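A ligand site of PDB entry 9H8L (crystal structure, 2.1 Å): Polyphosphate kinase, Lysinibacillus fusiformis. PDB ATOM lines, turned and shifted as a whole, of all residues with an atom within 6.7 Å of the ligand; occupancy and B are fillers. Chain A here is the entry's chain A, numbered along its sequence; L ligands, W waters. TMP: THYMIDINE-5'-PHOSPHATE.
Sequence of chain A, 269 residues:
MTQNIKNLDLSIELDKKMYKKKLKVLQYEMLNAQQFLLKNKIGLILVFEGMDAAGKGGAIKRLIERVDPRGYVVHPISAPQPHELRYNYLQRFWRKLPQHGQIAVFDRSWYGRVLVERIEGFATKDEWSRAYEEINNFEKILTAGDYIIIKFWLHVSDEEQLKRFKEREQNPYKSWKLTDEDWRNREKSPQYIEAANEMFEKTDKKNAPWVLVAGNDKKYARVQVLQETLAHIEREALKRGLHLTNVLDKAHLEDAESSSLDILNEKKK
The guanidinium group (NH1) of Arg 108 is in salt-bridge range of an oxygen (O1P) of the ligand (2.9 Å). A nitrogen (N3) of the ligand is in hydrogen-bond range of the side-chain carboxylate (OE2) of Glu 117 (3.0 Å).
The backbone NH of Phe 122 lies within hydrogen-bond range of the backbone carbonyl oxygen of Glu 117. The backbone NH (N) of Glu 117 lies within hydrogen-bond range of the backbone carbonyl oxygen (O) of Gly 112, at 3.0 Å. The backbone carbonyl oxygen (O) of Ser 78 is in hydrogen-bond range of the guanidinium group (NH2) of Arg 92, at 2.5 Å. The backbone NH of Ile 77 lies within hydrogen-bond range of the backbone carbonyl oxygen of Asp 107 (3.1 Å).
Ile 77 touches the ligand (O to C5M, 3.8 Å). Ser 78 touches the ligand (C to C5M, 3.8 Å). Ala 79 touches the ligand (CB to O4', 3.0 Å). CD of Pro 80 touches N3 of the ligand (3.8 Å). CG2 of Val 116 touches C2' of the ligand, at 3.6 Å. CD2 of Phe 122 touches O2 of the ligand, 3.2 Å away. Hydrophobic or aromatic side chains within 4 Å of the ligand: Ala 79, Pro 80, Val 116 and Phe 122. Eight residues have an atom within 4 Å of the ligand: Ile 77, Ser 78, Ala 79, Pro 80, Arg 108, Val 116, Glu 117 and Phe 122. The nearest printed residue that does not touch the ligand is Arg 92 (4.1 Å).
Water W1 bridges O4 of the ligand (2.7 Å) and O of Ser 109 (2.7 Å). Water W2 lies within hydrogen-bond range of the guanidinium group of Arg 108 (2.6 Å), an oxygen (O2P) of the ligand (2.8 Å) and the backbone carbonyl oxygen of Ile 77 (3.2 Å).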
ATOM      1  N   ASP A  52      16.498 -27.724   3.687  1.00  0.00           N
ATOM      2  CA  ASP A  52      17.410 -27.056   2.769  1.00  0.00           C
ATOM      3  C   ASP A  52      16.670 -26.660   1.484  1.00  0.00           C
ATOM      4  O   ASP A  52      15.898 -27.444   0.935  1.00  0.00           O
ATOM      5  CB  ASP A  52      18.592 -27.976   2.469  1.00  0.00           C
ATOM      6  CG  ASP A  52      19.805 -27.224   1.957  1.00  0.00           C
ATOM      7  OD1 ASP A  52      19.737 -25.983   1.845  1.00  0.00           O
ATOM      8  OD2 ASP A  52      20.834 -27.882   1.662  1.00  0.00           O
ATOM      9  N   ILE A  77      22.341 -19.850  11.734  1.00  0.00           N
ATOM     10  CA  ILE A  77      22.700 -20.807  12.765  1.00  0.00           C
ATOM     11  C   ILE A  77      23.187 -22.091  12.117  1.00  0.00           C
ATOM     12  O   ILE A  77      22.533 -22.640  11.223  1.00  0.00           O
ATOM     13  CB  ILE A  77      21.517 -21.066  13.703  1.00  0.00           C
ATOM     14  CG1 ILE A  77      21.147 -19.778  14.469  1.00  0.00           C
ATOM     15  CG2 ILE A  77      21.813 -22.229  14.640  1.00  0.00           C
ATOM     16  CD1 ILE A  77      22.279 -19.190  15.311  1.00  0.00           C
ATOM     17  N   SER A  78      24.347 -22.572  12.560  1.00  0.00           N
ATOM     18  CA  SER A  78      24.877 -23.863  12.121  1.00  0.00           C
ATOM     19  C   SER A  78      25.121 -24.747  13.351  1.00  0.00           C
ATOM     20  O   SER A  78      24.676 -24.441  14.457  1.00  0.00           O
ATOM     21  CB  SER A  78      26.148 -23.658  11.292  1.00  0.00           C
ATOM     22  OG  SER A  78      27.016 -22.720  11.903  1.00  0.00           O
ATOM     23  N   ALA A  79      25.864 -25.837  13.133  1.00  0.00           N
ATOM     24  CA  ALA A  79      26.135 -26.791  14.200  1.00  0.00           C
ATOM     25  C   ALA A  79      26.856 -26.117  15.360  1.00  0.00           C
ATOM     26  O   ALA A  79      27.700 -25.231  15.156  1.00  0.00           O
ATOM     27  CB  ALA A  79      26.989 -27.942  13.677  1.00  0.00           C
ATOM     28  N   PRO A  80      26.573 -26.533  16.590  1.00  0.00           N
ATOM     29  CA  PRO A  80      27.330 -26.026  17.742  1.00  0.00           C
ATOM     30  C   PRO A  80      28.826 -26.286  17.586  1.00  0.00           C
ATOM     31  O   PRO A  80      29.243 -27.371  17.171  1.00  0.00           O
ATOM     32  CB  PRO A  80      26.743 -26.805  18.926  1.00  0.00           C
ATOM     33  CG  PRO A  80      25.440 -27.367  18.439  1.00  0.00           C
ATOM     34  CD  PRO A  80      25.600 -27.578  16.971  1.00  0.00           C
ATOM     35  N   ARG A  92      23.982 -20.774  23.626  1.00  0.00           N
ATOM     36  CA  ARG A  92      24.397 -20.059  22.423  1.00  0.00           C
ATOM     37  C   ARG A  92      23.267 -19.204  21.855  1.00  0.00           C
ATOM     38  O   ARG A  92      23.521 -18.263  21.111  1.00  0.00           O
ATOM     39  CB  ARG A  92      24.882 -21.045  21.356  1.00  0.00           C
ATOM     40  CG  ARG A  92      23.759 -21.912  20.792  1.00  0.00           C
ATOM     41  CD  ARG A  92      24.268 -23.202  20.123  1.00  0.00           C
ATOM     42  NE  ARG A  92      24.750 -22.933  18.790  1.00  0.00           N
ATOM     43  CZ  ARG A  92      24.245 -23.424  17.672  1.00  0.00           C
ATOM     44  NH1 ARG A  92      23.299 -24.360  17.679  1.00  0.00           N
ATOM     45  NH2 ARG A  92      24.717 -22.988  16.511  1.00  0.00           N
ATOM     46  N   PHE A  93      22.022 -19.518  22.200  1.00  0.00           N
ATOM     47  CA  PHE A  93      20.891 -18.726  21.741  1.00  0.00           C
ATOM     48  C   PHE A  93      20.562 -17.600  22.725  1.00  0.00           C
ATOM     49  O   PHE A  93      20.304 -16.467  22.291  1.00  0.00           O
ATOM     50  CB  PHE A  93      19.700 -19.643  21.490  1.00  0.00           C
ATOM     51  CG  PHE A  93      19.970 -20.650  20.384  1.00  0.00           C
ATOM     52  CD1 PHE A  93      20.069 -20.232  19.064  1.00  0.00           C
ATOM     53  CD2 PHE A  93      20.179 -21.994  20.685  1.00  0.00           C
ATOM     54  CE1 PHE A  93      20.357 -21.144  18.043  1.00  0.00           C
ATOM     55  CE2 PHE A  93      20.471 -22.914  19.661  1.00  0.00           C
ATOM     56  CZ  PHE A  93      20.549 -22.498  18.348  1.00  0.00           C
ATOM     57  N   ASP A 107      17.864 -17.851  11.434  1.00  0.00           N
ATOM     58  CA  ASP A 107      17.769 -18.765  10.292  1.00  0.00           C
ATOM     59  C   ASP A 107      18.213 -20.130  10.812  1.00  0.00           C
ATOM     60  O   ASP A 107      19.409 -20.431  10.855  1.00  0.00           O
ATOM     61  CB  ASP A 107      18.617 -18.253   9.136  1.00  0.00           C
ATOM     62  CG  ASP A 107      18.440 -19.056   7.860  1.00  0.00           C
ATOM     63  OD1 ASP A 107      17.846 -20.147   7.899  1.00  0.00           O
ATOM     64  OD2 ASP A 107      18.903 -18.598   6.793  1.00  0.00           O
ATOM     65  N   ARG A 108      17.232 -20.937  11.234  1.00  0.00           N
ATOM     66  CA  ARG A 108      17.400 -22.096  12.113  1.00  0.00           C
ATOM     67  C   ARG A 108      17.731 -21.613  13.516  1.00  0.00           C
ATOM     68  O   ARG A 108      18.139 -20.458  13.702  1.00  0.00           O
ATOM     69  CB  ARG A 108      18.457 -23.073  11.571  1.00  0.00           C
ATOM     70  CG  ARG A 108      18.144 -23.516  10.145  1.00  0.00           C
ATOM     71  CD  ARG A 108      19.190 -24.466   9.579  1.00  0.00           C
ATOM     72  NE  ARG A 108      19.017 -25.843  10.015  1.00  0.00           N
ATOM     73  CZ  ARG A 108      19.696 -26.866   9.517  1.00  0.00           C
ATOM     74  NH1 ARG A 108      20.581 -26.691   8.542  1.00  0.00           N
ATOM     75  NH2 ARG A 108      19.484 -28.093  10.002  1.00  0.00           N
ATOM     76  N   SER A 109      17.516 -22.465  14.520  1.00  0.00           N
ATOM     77  CA  SER A 109      17.308 -21.937  15.850  1.00  0.00           C
ATOM     78  C   SER A 109      17.505 -23.045  16.889  1.00  0.00           C
ATOM     79  O   SER A 109      18.061 -24.111  16.574  1.00  0.00           O
ATOM     80  CB  SER A 109      15.896 -21.323  15.942  1.00  0.00           C
ATOM     81  OG  SER A 109      14.911 -22.341  15.897  1.00  0.00           O
ATOM     82  N   TYR A 111      15.304 -24.928  17.840  1.00  0.00           N
ATOM     83  CA  TYR A 111      14.515 -26.075  17.403  1.00  0.00           C
ATOM     84  C   TYR A 111      15.355 -27.133  16.695  1.00  0.00           C
ATOM     85  O   TYR A 111      14.847 -28.241  16.468  1.00  0.00           O
ATOM     86  CB  TYR A 111      13.344 -25.618  16.515  1.00  0.00           C
ATOM     87  CG  TYR A 111      12.258 -24.968  17.321  1.00  0.00           C
ATOM     88  CD1 TYR A 111      11.288 -25.735  17.974  1.00  0.00           C
ATOM     89  CD2 TYR A 111      12.204 -23.593  17.475  1.00  0.00           C
ATOM     90  CE1 TYR A 111      10.290 -25.133  18.737  1.00  0.00           C
ATOM     91  CE2 TYR A 111      11.219 -22.980  18.224  1.00  0.00           C
ATOM     92  CZ  TYR A 111      10.270 -23.753  18.857  1.00  0.00           C
ATOM     93  OH  TYR A 111       9.301 -23.145  19.610  1.00  0.00           O
ATOM     94  N   GLY A 112      16.616 -26.839  16.362  1.00  0.00           N
ATOM     95  CA  GLY A 112      17.517 -27.889  15.913  1.00  0.00           C
ATOM     96  C   GLY A 112      17.590 -29.030  16.909  1.00  0.00           C
ATOM     97  O   GLY A 112      17.804 -30.187  16.520  1.00  0.00           O
ATOM     98  N   ARG A 113      17.361 -28.739  18.188  1.00  0.00           N
ATOM     99  CA  ARG A 113      17.347 -29.780  19.212  1.00  0.00           C
ATOM    100  C   ARG A 113      16.316 -30.871  18.913  1.00  0.00           C
ATOM    101  O   ARG A 113      16.523 -32.031  19.287  1.00  0.00           O
ATOM    102  CB  ARG A 113      17.076 -29.161  20.593  1.00  0.00           C
ATOM    103  CG  ARG A 113      17.179 -30.140  21.766  1.00  0.00           C
ATOM    104  CD  ARG A 113      18.620 -30.381  22.179  1.00  0.00           C
ATOM    105  NE  ARG A 113      18.746 -30.725  23.596  1.00  0.00           N
ATOM    106  CZ  ARG A 113      19.892 -31.022  24.193  1.00  0.00           C
ATOM    107  NH1 ARG A 113      21.035 -31.050  23.519  1.00  0.00           N
ATOM    108  NH2 ARG A 113      19.894 -31.315  25.494  1.00  0.00           N
ATOM    109  N   VAL A 116      17.215 -31.636  13.335  1.00  0.00           N
ATOM    110  CA  VAL A 116      18.392 -32.347  12.832  1.00  0.00           C
ATOM    111  C   VAL A 116      19.092 -33.110  13.944  1.00  0.00           C
ATOM    112  O   VAL A 116      19.585 -34.219  13.734  1.00  0.00           O
ATOM    113  CB  VAL A 116      19.351 -31.367  12.119  1.00  0.00           C
ATOM    114  CG1 VAL A 116      19.852 -30.292  13.093  1.00  0.00           C
ATOM    115  CG2 VAL A 116      20.516 -32.123  11.527  1.00  0.00           C
ATOM    116  N   GLU A 117      19.123 -32.541  15.153  1.00  0.00           N
ATOM    117  CA  GLU A 117      19.817 -33.220  16.249  1.00  0.00           C
ATOM    118  C   GLU A 117      19.047 -34.442  16.717  1.00  0.00           C
ATOM    119  O   GLU A 117      19.653 -35.426  17.168  1.00  0.00           O
ATOM    120  CB  GLU A 117      20.067 -32.236  17.406  1.00  0.00           C
ATOM    121  CG  GLU A 117      21.006 -31.090  16.989  1.00  0.00           C
ATOM    122  CD  GLU A 117      21.229 -30.028  18.049  1.00  0.00           C
ATOM    123  OE1 GLU A 117      20.937 -30.262  19.247  1.00  0.00           O
ATOM    124  OE2 GLU A 117      21.720 -28.937  17.670  1.00  0.00           O
ATOM    125  N   GLU A 120      19.565 -37.030  13.554  1.00  0.00           N
ATOM    126  CA  GLU A 120      20.910 -37.555  13.416  1.00  0.00           C
ATOM    127  C   GLU A 120      21.375 -38.294  14.668  1.00  0.00           C
ATOM    128  O   GLU A 120      22.477 -38.845  14.666  1.00  0.00           O
ATOM    129  CB  GLU A 120      21.882 -36.430  13.070  1.00  0.00           C
ATOM    130  CG  GLU A 120      21.664 -35.836  11.674  1.00  0.00           C
ATOM    131  CD  GLU A 120      21.868 -36.875  10.568  1.00  0.00           C
ATOM    132  OE1 GLU A 120      22.929 -37.530  10.543  1.00  0.00           O
ATOM    133  OE2 GLU A 120      20.967 -37.022   9.716  1.00  0.00           O
ATOM    134  N   PHE A 122      22.251 -36.866  17.410  1.00  0.00           N
ATOM    135  CA  PHE A 122      23.166 -36.039  18.202  1.00  0.00           C
ATOM    136  C   PHE A 122      22.605 -35.775  19.597  1.00  0.00           C
ATOM    137  O   PHE A 122      23.347 -35.775  20.586  1.00  0.00           O
ATOM    138  CB  PHE A 122      23.466 -34.707  17.502  1.00  0.00           C
ATOM    139  CG  PHE A 122      24.105 -34.841  16.141  1.00  0.00           C
ATOM    140  CD1 PHE A 122      24.828 -35.980  15.803  1.00  0.00           C
ATOM    141  CD2 PHE A 122      23.984 -33.835  15.197  1.00  0.00           C
ATOM    142  CE1 PHE A 122      25.409 -36.108  14.541  1.00  0.00           C
ATOM    143  CE2 PHE A 122      24.564 -33.955  13.948  1.00  0.00           C
ATOM    144  CZ  PHE A 122      25.275 -35.091  13.615  1.00  0.00           C
ATOM    145  N   LYS A 177      28.770 -24.725  -2.508  1.00  0.00           N
ATOM    146  CA  LYS A 177      28.223 -25.106  -1.211  1.00  0.00           C
ATOM    147  C   LYS A 177      27.378 -26.376  -1.242  1.00  0.00           C
ATOM    148  O   LYS A 177      27.167 -26.986  -0.191  1.00  0.00           O
ATOM    149  CB  LYS A 177      27.379 -23.952  -0.648  1.00  0.00           C
ATOM    150  CG  LYS A 177      27.023 -24.073   0.833  1.00  0.00           C
ATOM    151  CD  LYS A 177      26.243 -22.856   1.336  1.00  0.00           C
ATOM    152  CE  LYS A 177      25.749 -23.095   2.766  1.00  0.00           C
ATOM    153  NZ  LYS A 177      24.921 -21.975   3.316  1.00  0.00           N
ATOM    154  N   GLU A 181      26.650 -34.824   0.305  1.00  0.00           N
ATOM    155  CA  GLU A 181      25.947 -35.117   1.536  1.00  0.00           C
ATOM    156  C   GLU A 181      24.555 -34.492   1.557  1.00  0.00           C
ATOM    157  O   GLU A 181      23.616 -35.086   2.094  1.00  0.00           O
ATOM    158  CB  GLU A 181      26.771 -34.640   2.733  1.00  0.00           C
ATOM    159  CG  GLU A 181      26.176 -35.015   4.082  1.00  0.00           C
ATOM    160  CD  GLU A 181      26.997 -34.521   5.261  1.00  0.00           C
ATOM    161  OE1 GLU A 181      28.191 -34.211   5.055  1.00  0.00           O
ATOM    162  OE2 GLU A 181      26.459 -34.439   6.379  1.00  0.00           O
ATOM    163  N   ASP A 182      24.395 -33.301   0.962  1.00  0.00           N
ATOM    164  CA  ASP A 182      23.075 -32.666   0.923  1.00  0.00           C
ATOM    165  C   ASP A 182      22.092 -33.485   0.083  1.00  0.00           C
ATOM    166  O   ASP A 182      20.935 -33.717   0.482  1.00  0.00           O
ATOM    167  CB  ASP A 182      23.201 -31.241   0.384  1.00  0.00           C
ATOM    168  CG  ASP A 182      24.195 -30.408   1.167  1.00  0.00           C
ATOM    169  OD1 ASP A 182      24.124 -30.402   2.414  1.00  0.00           O
ATOM    170  OD2 ASP A 182      25.068 -29.768   0.543  1.00  0.00           O
ATOM    171  N   ASN A 185      21.145 -36.459   2.114  1.00  0.00           N
ATOM    172  CA  ASN A 185      20.237 -36.059   3.179  1.00  0.00           C
ATOM    173  C   ASN A 185      18.819 -35.859   2.685  1.00  0.00           C
ATOM    174  O   ASN A 185      17.886 -35.894   3.494  1.00  0.00           O
ATOM    175  CB  ASN A 185      20.710 -34.756   3.830  1.00  0.00           C
ATOM    176  CG  ASN A 185      21.791 -34.982   4.867  1.00  0.00           C
ATOM    177  OD1 ASN A 185      22.232 -36.113   5.077  1.00  0.00           O
ATOM    178  ND2 ASN A 185      22.230 -33.912   5.506  1.00  0.00           N
ATOM    179  N   TYR A 192      12.362 -35.947   8.837  1.00  0.00           N
ATOM    180  CA  TYR A 192      12.276 -34.532   9.162  1.00  0.00           C
ATOM    181  C   TYR A 192      10.832 -34.069   9.210  1.00  0.00           C
ATOM    182  O   TYR A 192      10.457 -33.257  10.065  1.00  0.00           O
ATOM    183  CB  TYR A 192      13.039 -33.673   8.161  1.00  0.00           C
ATOM    184  CG  TYR A 192      14.489 -33.506   8.483  1.00  0.00           C
ATOM    185  CD1 TYR A 192      14.925 -32.503   9.341  1.00  0.00           C
ATOM    186  CD2 TYR A 192      15.429 -34.365   7.941  1.00  0.00           C
ATOM    187  CE1 TYR A 192      16.261 -32.359   9.639  1.00  0.00           C
ATOM    188  CE2 TYR A 192      16.770 -34.237   8.224  1.00  0.00           C
ATOM    189  CZ  TYR A 192      17.181 -33.233   9.081  1.00  0.00           C
ATOM    190  OH  TYR A 192      18.527 -33.121   9.349  1.00  0.00           O
HETATM  191  P   TMP L   1      24.408 -27.860   7.906  1.00  0.00           P
HETATM  192  O1P TMP L   1      22.947 -28.037   7.564  1.00  0.00           O
HETATM  193  O2P TMP L   1      24.709 -26.534   8.586  1.00  0.00           O
HETATM  194  O3P TMP L   1      25.327 -28.133   6.726  1.00  0.00           O
HETATM  195  O5' TMP L   1      24.721 -29.013   9.000  1.00  0.00           O
HETATM  196  C5' TMP L   1      26.097 -29.364   9.302  1.00  0.00           C
HETATM  197  C4' TMP L   1      26.107 -30.379  10.418  1.00  0.00           C
HETATM  198  O4' TMP L   1      25.704 -29.750  11.657  1.00  0.00           O
HETATM  199  C3' TMP L   1      25.188 -31.583  10.231  1.00  0.00           C
HETATM  200  O3' TMP L   1      25.827 -32.756  10.736  1.00  0.00           O
HETATM  201  C2' TMP L   1      23.979 -31.230  11.081  1.00  0.00           C
HETATM  202  C1' TMP L   1      24.624 -30.472  12.230  1.00  0.00           C
HETATM  203  N1  TMP L   1      23.727 -29.492  12.916  1.00  0.00           N
HETATM  204  C2  TMP L   1      23.478 -29.686  14.256  1.00  0.00           C
HETATM  205  O2  TMP L   1      23.889 -30.659  14.873  1.00  0.00           O
HETATM  206  N3  TMP L   1      22.709 -28.711  14.836  1.00  0.00           N
HETATM  207  C4  TMP L   1      22.177 -27.589  14.225  1.00  0.00           C
HETATM  208  O4  TMP L   1      21.505 -26.782  14.882  1.00  0.00           O
HETATM  209  C5  TMP L   1      22.474 -27.452  12.814  1.00  0.00           C
HETATM  210  C5M TMP L   1      21.924 -26.268  12.069  1.00  0.00           C
HETATM  211  C6  TMP L   1      23.218 -28.404  12.237  1.00  0.00           C
HETATM  212  O   HOH W   1      19.273 -25.292  14.438  1.00  0.00           O
HETATM  213  O   HOH W   2      22.456 -24.872   8.885  1.00  0.00           O
